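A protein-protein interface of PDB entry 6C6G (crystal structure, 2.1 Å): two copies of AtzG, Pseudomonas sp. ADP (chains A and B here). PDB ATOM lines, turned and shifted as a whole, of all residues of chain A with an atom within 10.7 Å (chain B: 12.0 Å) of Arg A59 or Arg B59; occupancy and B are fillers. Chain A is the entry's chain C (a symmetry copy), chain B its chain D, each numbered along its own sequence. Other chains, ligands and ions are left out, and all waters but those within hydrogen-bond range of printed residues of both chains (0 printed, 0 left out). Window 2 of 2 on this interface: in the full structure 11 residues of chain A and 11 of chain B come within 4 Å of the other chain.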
ATOM      1  N   GLU A  53     -12.068  34.290   6.662  1.00  0.00           N
ATOM      2  CA  GLU A  53     -11.956  33.498   5.444  1.00  0.00           C
ATOM      3  C   GLU A  53     -12.307  34.235   4.129  1.00  0.00           C
ATOM      4  O   GLU A  53     -12.855  35.315   4.094  1.00  0.00           O
ATOM      5  CB  GLU A  53     -12.846  32.227   5.574  1.00  0.00           C
ATOM      6  CG  GLU A  53     -12.567  31.400   6.840  1.00  0.00           C
ATOM      7  CD  GLU A  53     -13.198  30.038   6.833  1.00  0.00           C
ATOM      8  OE1 GLU A  53     -13.424  29.524   5.742  1.00  0.00           O
ATOM      9  OE2 GLU A  53     -13.509  29.478   7.914  1.00  0.00           O
ATOM     10  N   LEU A  54     -11.959  33.587   3.049  1.00  0.00           N
ATOM     11  CA  LEU A  54     -12.279  34.020   1.704  1.00  0.00           C
ATOM     12  C   LEU A  54     -13.807  34.133   1.607  1.00  0.00           C
ATOM     13  O   LEU A  54     -14.526  33.361   2.239  1.00  0.00           O
ATOM     14  CB  LEU A  54     -11.788  32.975   0.684  1.00  0.00           C
ATOM     15  CG  LEU A  54     -10.296  32.592   0.584  1.00  0.00           C
ATOM     16  CD1 LEU A  54     -10.072  31.294  -0.157  1.00  0.00           C
ATOM     17  CD2 LEU A  54      -9.499  33.709  -0.043  1.00  0.00           C
ATOM     18  N   ALA A  55     -14.285  35.094   0.812  1.00  0.00           N
ATOM     19  CA  ALA A  55     -15.706  35.239   0.569  1.00  0.00           C
ATOM     20  C   ALA A  55     -16.356  33.967   0.017  1.00  0.00           C
ATOM     21  O   ALA A  55     -17.524  33.709   0.335  1.00  0.00           O
ATOM     22  CB  ALA A  55     -15.999  36.420  -0.374  1.00  0.00           C
ATOM     23  N   GLU A  56     -15.656  33.205  -0.803  1.00  0.00           N
ATOM     24  CA  GLU A  56     -16.226  31.953  -1.304  1.00  0.00           C
ATOM     25  C   GLU A  56     -15.349  30.730  -1.045  1.00  0.00           C
ATOM     26  O   GLU A  56     -14.162  30.707  -1.417  1.00  0.00           O
ATOM     27  CB  GLU A  56     -16.633  32.083  -2.786  1.00  0.00           C
ATOM     28  CG  GLU A  56     -17.736  33.132  -3.061  1.00  0.00           C
ATOM     29  CD  GLU A  56     -19.057  32.854  -2.296  1.00  0.00           C
ATOM     30  OE1 GLU A  56     -19.370  31.680  -1.969  1.00  0.00           O
ATOM     31  OE2 GLU A  56     -19.806  33.799  -2.045  1.00  0.00           O
ATOM     32  N   ILE A  57     -15.942  29.747  -0.371  1.00  0.00           N
ATOM     33  CA  ILE A  57     -15.264  28.513  -0.032  1.00  0.00           C
ATOM     34  C   ILE A  57     -15.832  27.332  -0.858  1.00  0.00           C
ATOM     35  O   ILE A  57     -17.051  27.217  -1.042  1.00  0.00           O
ATOM     36  CB  ILE A  57     -15.380  28.202   1.493  1.00  0.00           C
ATOM     37  CG1 ILE A  57     -14.862  29.371   2.368  1.00  0.00           C
ATOM     38  CG2 ILE A  57     -14.606  26.931   1.863  1.00  0.00           C
ATOM     39  CD1 ILE A  57     -13.470  29.845   2.004  1.00  0.00           C
ATOM     40  N   TYR A  58     -14.925  26.484  -1.354  1.00  0.00           N
ATOM     41  CA  TYR A  58     -15.260  25.324  -2.154  1.00  0.00           C
ATOM     42  C   TYR A  58     -16.456  24.461  -1.698  1.00  0.00           C
ATOM     43  O   TYR A  58     -16.632  24.173  -0.508  1.00  0.00           O
ATOM     44  CB  TYR A  58     -14.048  24.418  -2.206  1.00  0.00           C
ATOM     45  CG  TYR A  58     -14.108  23.281  -3.189  1.00  0.00           C
ATOM     46  CD1 TYR A  58     -14.057  23.543  -4.558  1.00  0.00           C
ATOM     47  CD2 TYR A  58     -14.117  21.955  -2.768  1.00  0.00           C
ATOM     48  CE1 TYR A  58     -14.041  22.524  -5.478  1.00  0.00           C
ATOM     49  CE2 TYR A  58     -14.094  20.920  -3.692  1.00  0.00           C
ATOM     50  CZ  TYR A  58     -14.043  21.210  -5.033  1.00  0.00           C
ATOM     51  OH  TYR A  58     -14.055  20.228  -5.953  1.00  0.00           O
ATOM     52  N   ARG A  59     -17.250  24.039  -2.686  1.00  0.00           N
ATOM     53  CA  ARG A  59     -18.322  23.099  -2.490  1.00  0.00           C
ATOM     54  C   ARG A  59     -18.065  21.899  -3.433  1.00  0.00           C
ATOM     55  O   ARG A  59     -18.101  22.064  -4.662  1.00  0.00           O
ATOM     56  CB  ARG A  59     -19.632  23.770  -2.820  1.00  0.00           C
ATOM     57  CG  ARG A  59     -19.964  24.947  -1.914  1.00  0.00           C
ATOM     58  CD  ARG A  59     -20.786  25.945  -2.690  1.00  0.00           C
ATOM     59  NE  ARG A  59     -21.348  27.026  -1.854  1.00  0.00           N
ATOM     60  CZ  ARG A  59     -21.024  28.331  -1.934  1.00  0.00           C
ATOM     61  NH1 ARG A  59     -20.132  28.805  -2.820  1.00  0.00           N
ATOM     62  NH2 ARG A  59     -21.607  29.194  -1.101  1.00  0.00           N
ATOM     63  N   PRO A  60     -17.783  20.706  -2.858  1.00  0.00           N
ATOM     64  CA  PRO A  60     -17.328  19.571  -3.659  1.00  0.00           C
ATOM     65  C   PRO A  60     -18.414  18.941  -4.547  1.00  0.00           C
ATOM     66  O   PRO A  60     -18.069  18.308  -5.539  1.00  0.00           O
ATOM     67  CB  PRO A  60     -16.804  18.584  -2.622  1.00  0.00           C
ATOM     68  CG  PRO A  60     -17.598  18.879  -1.404  1.00  0.00           C
ATOM     69  CD  PRO A  60     -17.908  20.355  -1.437  1.00  0.00           C
ATOM     70  N   ALA A  61     -19.665  19.141  -4.172  1.00  0.00           N
ATOM     71  CA  ALA A  61     -20.886  18.630  -4.829  1.00  0.00           C
ATOM     72  C   ALA A  61     -22.058  19.074  -3.954  1.00  0.00           C
ATOM     73  O   ALA A  61     -21.886  19.234  -2.759  1.00  0.00           O
ATOM     74  CB  ALA A  61     -20.919  17.111  -4.959  1.00  0.00           C
ATOM     75  N   PRO A  62     -23.265  19.252  -4.540  1.00  0.00           N
ATOM     76  CA  PRO A  62     -24.418  19.629  -3.718  1.00  0.00           C
ATOM     77  C   PRO A  62     -24.723  18.569  -2.667  1.00  0.00           C
ATOM     78  O   PRO A  62     -24.511  17.387  -2.897  1.00  0.00           O
ATOM     79  CB  PRO A  62     -25.562  19.716  -4.730  1.00  0.00           C
ATOM     80  CG  PRO A  62     -25.118  18.893  -5.885  1.00  0.00           C
ATOM     81  CD  PRO A  62     -23.635  19.024  -5.944  1.00  0.00           C
ATOM     82  N   PHE A  63     -25.182  19.022  -1.513  1.00  0.00           N
ATOM     83  CA  PHE A  63     -25.606  18.130  -0.441  1.00  0.00           C
ATOM     84  C   PHE A  63     -26.867  17.343  -0.854  1.00  0.00           C
ATOM     85  O   PHE A  63     -27.817  17.932  -1.288  1.00  0.00           O
ATOM     86  CB  PHE A  63     -25.878  18.894   0.860  1.00  0.00           C
ATOM     87  CG  PHE A  63     -25.879  17.996   2.085  1.00  0.00           C
ATOM     88  CD1 PHE A  63     -24.667  17.570   2.628  1.00  0.00           C
ATOM     89  CD2 PHE A  63     -27.076  17.560   2.682  1.00  0.00           C
ATOM     90  CE1 PHE A  63     -24.628  16.756   3.763  1.00  0.00           C
ATOM     91  CE2 PHE A  63     -27.035  16.703   3.798  1.00  0.00           C
ATOM     92  CZ  PHE A  63     -25.801  16.301   4.334  1.00  0.00           C
ATOM     93  N   GLU B  53     -14.963  29.170 -15.797  1.00  0.00           N
ATOM     94  CA  GLU B  53     -14.971  30.008 -14.611  1.00  0.00           C
ATOM     95  C   GLU B  53     -14.233  29.403 -13.382  1.00  0.00           C
ATOM     96  O   GLU B  53     -13.912  28.199 -13.315  1.00  0.00           O
ATOM     97  CB  GLU B  53     -16.418  30.380 -14.237  1.00  0.00           C
ATOM     98  CG  GLU B  53     -17.192  31.068 -15.371  1.00  0.00           C
ATOM     99  CD  GLU B  53     -18.415  31.884 -14.877  1.00  0.00           C
ATOM    100  OE1 GLU B  53     -18.468  32.191 -13.673  1.00  0.00           O
ATOM    101  OE2 GLU B  53     -19.362  32.166 -15.655  1.00  0.00           O
ATOM    102  N   LEU B  54     -14.014  30.269 -12.410  1.00  0.00           N
ATOM    103  CA  LEU B  54     -13.507  29.884 -11.129  1.00  0.00           C
ATOM    104  C   LEU B  54     -14.435  28.842 -10.513  1.00  0.00           C
ATOM    105  O   LEU B  54     -15.631  28.847 -10.753  1.00  0.00           O
ATOM    106  CB  LEU B  54     -13.462  31.135 -10.225  1.00  0.00           C
ATOM    107  CG  LEU B  54     -12.527  32.313 -10.536  1.00  0.00           C
ATOM    108  CD1 LEU B  54     -12.885  33.494  -9.678  1.00  0.00           C
ATOM    109  CD2 LEU B  54     -11.083  31.894 -10.283  1.00  0.00           C
ATOM    110  N   ALA B  55     -13.865  27.952  -9.722  1.00  0.00           N
ATOM    111  CA  ALA B  55     -14.632  26.933  -8.993  1.00  0.00           C
ATOM    112  C   ALA B  55     -15.759  27.511  -8.158  1.00  0.00           C
ATOM    113  O   ALA B  55     -16.805  26.879  -8.007  1.00  0.00           O
ATOM    114  CB  ALA B  55     -13.712  26.105  -8.080  1.00  0.00           C
ATOM    115  N   GLU B  56     -15.541  28.688  -7.560  1.00  0.00           N
ATOM    116  CA  GLU B  56     -16.578  29.283  -6.723  1.00  0.00           C
ATOM    117  C   GLU B  56     -16.789  30.754  -7.108  1.00  0.00           C
ATOM    118  O   GLU B  56     -15.816  31.543  -7.190  1.00  0.00           O
ATOM    119  CB  GLU B  56     -16.229  29.140  -5.241  1.00  0.00           C
ATOM    120  CG  GLU B  56     -16.101  27.692  -4.734  1.00  0.00           C
ATOM    121  CD  GLU B  56     -17.399  26.898  -4.869  1.00  0.00           C
ATOM    122  OE1 GLU B  56     -18.483  27.469  -4.867  1.00  0.00           O
ATOM    123  OE2 GLU B  56     -17.379  25.673  -4.969  1.00  0.00           O
ATOM    124  N   ILE B  57     -18.052  31.120  -7.342  1.00  0.00           N
ATOM    125  CA  ILE B  57     -18.392  32.494  -7.725  1.00  0.00           C
ATOM    126  C   ILE B  57     -19.195  33.167  -6.588  1.00  0.00           C
ATOM    127  O   ILE B  57     -20.046  32.541  -5.968  1.00  0.00           O
ATOM    128  CB  ILE B  57     -19.214  32.526  -9.062  1.00  0.00           C
ATOM    129  CG1 ILE B  57     -18.494  31.775 -10.201  1.00  0.00           C
ATOM    130  CG2 ILE B  57     -19.521  33.965  -9.497  1.00  0.00           C
ATOM    131  CD1 ILE B  57     -17.088  32.241 -10.458  1.00  0.00           C
ATOM    132  N   TYR B  58     -18.920  34.442  -6.343  1.00  0.00           N
ATOM    133  CA  TYR B  58     -19.588  35.230  -5.304  1.00  0.00           C
ATOM    134  C   TYR B  58     -21.116  35.094  -5.193  1.00  0.00           C
ATOM    135  O   TYR B  58     -21.835  35.049  -6.208  1.00  0.00           O
ATOM    136  CB  TYR B  58     -19.260  36.690  -5.558  1.00  0.00           C
ATOM    137  CG  TYR B  58     -19.670  37.658  -4.502  1.00  0.00           C
ATOM    138  CD1 TYR B  58     -19.006  37.688  -3.301  1.00  0.00           C
ATOM    139  CD2 TYR B  58     -20.651  38.633  -4.738  1.00  0.00           C
ATOM    140  CE1 TYR B  58     -19.293  38.639  -2.342  1.00  0.00           C
ATOM    141  CE2 TYR B  58     -20.968  39.583  -3.768  1.00  0.00           C
ATOM    142  CZ  TYR B  58     -20.273  39.586  -2.594  1.00  0.00           C
ATOM    143  OH  TYR B  58     -20.561  40.470  -1.618  1.00  0.00           O
ATOM    144  N   ARG B  59     -21.591  35.079  -3.954  1.00  0.00           N
ATOM    145  CA  ARG B  59     -23.003  35.135  -3.638  1.00  0.00           C
ATOM    146  C   ARG B  59     -23.218  36.338  -2.700  1.00  0.00           C
ATOM    147  O   ARG B  59     -22.701  36.347  -1.574  1.00  0.00           O
ATOM    148  CB  ARG B  59     -23.429  33.855  -2.947  1.00  0.00           C
ATOM    149  CG  ARG B  59     -23.227  32.606  -3.814  1.00  0.00           C
ATOM    150  CD  ARG B  59     -22.908  31.457  -2.916  1.00  0.00           C
ATOM    151  NE  ARG B  59     -22.748  30.182  -3.624  1.00  0.00           N
ATOM    152  CZ  ARG B  59     -23.735  29.388  -4.040  1.00  0.00           C
ATOM    153  NH1 ARG B  59     -25.023  29.749  -3.920  1.00  0.00           N
ATOM    154  NH2 ARG B  59     -23.417  28.224  -4.622  1.00  0.00           N
ATOM    155  N   PRO B  60     -23.968  37.357  -3.169  1.00  0.00           N
ATOM    156  CA  PRO B  60     -24.066  38.635  -2.428  1.00  0.00           C
ATOM    157  C   PRO B  60     -24.886  38.548  -1.146  1.00  0.00           C
ATOM    158  O   PRO B  60     -24.655  39.350  -0.242  1.00  0.00           O
ATOM    159  CB  PRO B  60     -24.718  39.584  -3.424  1.00  0.00           C
ATOM    160  CG  PRO B  60     -25.524  38.698  -4.320  1.00  0.00           C
ATOM    161  CD  PRO B  60     -24.800  37.363  -4.389  1.00  0.00           C
ATOM    162  N   ALA B  61     -25.784  37.567  -1.084  1.00  0.00           N
ATOM    163  CA  ALA B  61     -26.641  37.241   0.075  1.00  0.00           C
ATOM    164  C   ALA B  61     -27.449  36.004  -0.319  1.00  0.00           C
ATOM    165  O   ALA B  61     -27.602  35.737  -1.494  1.00  0.00           O
ATOM    166  CB  ALA B  61     -27.582  38.396   0.382  1.00  0.00           C
ATOM    167  N   PRO B  62     -27.988  35.248   0.649  1.00  0.00           N
ATOM    168  CA  PRO B  62     -28.818  34.087   0.297  1.00  0.00           C
ATOM    169  C   PRO B  62     -30.040  34.523  -0.463  1.00  0.00           C
ATOM    170  O   PRO B  62     -30.566  35.616  -0.203  1.00  0.00           O
ATOM    171  CB  PRO B  62     -29.245  33.509   1.660  1.00  0.00           C
ATOM    172  CG  PRO B  62     -28.224  34.047   2.612  1.00  0.00           C
ATOM    173  CD  PRO B  62     -27.877  35.411   2.107  1.00  0.00           C
ATOM    174  N   PHE B  63     -30.479  33.704  -1.414  1.00  0.00           N
ATOM    175  CA  PHE B  63     -31.699  34.004  -2.162  1.00  0.00           C
ATOM    176  C   PHE B  63     -32.916  33.865  -1.226  1.00  0.00           C
ATOM    177  O   PHE B  63     -33.035  32.864  -0.533  1.00  0.00           O
ATOM    178  CB  PHE B  63     -31.876  33.070  -3.364  1.00  0.00           C
ATOM    179  CG  PHE B  63     -32.906  33.590  -4.364  1.00  0.00           C
ATOM    180  CD1 PHE B  63     -32.586  34.680  -5.218  1.00  0.00           C
ATOM    181  CD2 PHE B  63     -34.200  33.050  -4.419  1.00  0.00           C
ATOM    182  CE1 PHE B  63     -33.524  35.194  -6.092  1.00  0.00           C
ATOM    183  CE2 PHE B  63     -35.133  33.565  -5.323  1.00  0.00           C
ATOM    184  CZ  PHE B  63     -34.801  34.654  -6.137  1.00  0.00           C
ATOM    185  N   PRO B  64     -33.820  34.859  -1.207  1.00  0.00           N
ATOM    186  CA  PRO B  64     -34.890  34.842  -0.186  1.00  0.00           C
ATOM    187  C   PRO B  64     -35.902  33.746  -0.391  1.00  0.00           C
ATOM    188  O   PRO B  64     -36.291  33.508  -1.525  1.00  0.00           O
ATOM    189  CB  PRO B  64     -35.542  36.214  -0.351  1.00  0.00           C
ATOM    190  CG  PRO B  64     -35.219  36.641  -1.747  1.00  0.00           C
ATOM    191  CD  PRO B  64     -33.926  36.008  -2.114  1.00  0.00           C
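The side-chain carboxylate of Glu B56 is in salt-bridge range of the guanidinium group of Arg A59 (2.9 Å).
The side-chain carboxylate (OE2) of Glu A56 is in hydrogen-bond range of the backbone NH (N) of Arg B59 (2.9 Å).
NH2 of Arg A59 sits close to NE of Arg B59 (2.9 Å).
The side-chain carboxylate (OE1) of Glu A56 lies within salt-bridge range of the guanidinium group (NH1) of Arg A59 (3.1 Å).
Among the printed residues, pairs that only touch across the chains: Tyr A58 with Glu B56 (3.5 Å), Glu A56 with Tyr B58 (3.6 Å), Glu A56 with Ile B57 (3.8 Å), Ile A57 with Glu B56 (3.8 Å) and Glu A56 with Glu B56 (3.9 Å).
Printed residues of chain B within 4 Å of Arg A59: Glu B56 (2.8 Å) and Arg B59 (2.9 Å).
Arg B59 touches just these residues of chain A: Glu A56 (2.9 Å) and Arg A59 (2.9 Å).
Of chain B, only Glu B56, Ile B57, Tyr B58 and Arg B59 come within 4 Å of Glu A56.
Tyr A58 touches one residue of chain B.
No residue of chain B comes within 4 Å of Pro A60.
Ala A61 touches none of the printed residues of chain B.
No residue of chain B comes within 4 Å of Pro A62.
Of chain A, only Glu A56 (3.6 Å) comes within 4 Å of Tyr B58.
No residue of chain A comes within 4 Å of Pro B60.
No residue of chain A comes within 4 Å of Ala B61.
Of the printed residues of chain B, Ile A57 touches Glu B56.
Printed residues of chain A within 4 Å of Ile B57: Glu A56 (3.8 Å).
Of the printed residues of chain A, Glu B56 touches Glu A56 (3.9 Å), Ile A57 (3.8 Å), Tyr A58 (3.5 Å) and Arg A59 (2.8 Å).
Pro B62 touches none of the printed residues of chain A.
Phe B63 touches none of the printed residues of chain A.
The nearest printed residue of chain B that does not touch Ile A57 is Arg B59 (6.9 Å).
Hydrophobic or aromatic side chains of chain A that line the printed part of chain B: Tyr A58.
Printed residues of chain B that touch a printed residue of chain A: Glu B56, Ile B57, Tyr B58 and Arg B59.
Among the printed residues, Asp or Glu carboxylates within 4 Å of a Lys or Arg side-chain nitrogen of the other chain: Arg A59 with Glu B56.
Glu A56 touches its own counterpart, Glu B56.
Glu A56 touches Ile B57, and with the chains exchanged Ile A57 touches Glu B56.
Glu A56 touches Tyr B58, and with the chains exchanged Tyr A58 touches Glu B56.
Glu A56 touches Arg B59, and with the chains exchanged Arg A59 touches Glu B56.
Positions printed for both chains: 53, 54, 55, 56, 57, 58, 59, 60, 61, 62 and 63.
Of the 8 pairs that touch across the chains among the printed residues, 8 have their exchanged pair printed and touching as well.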
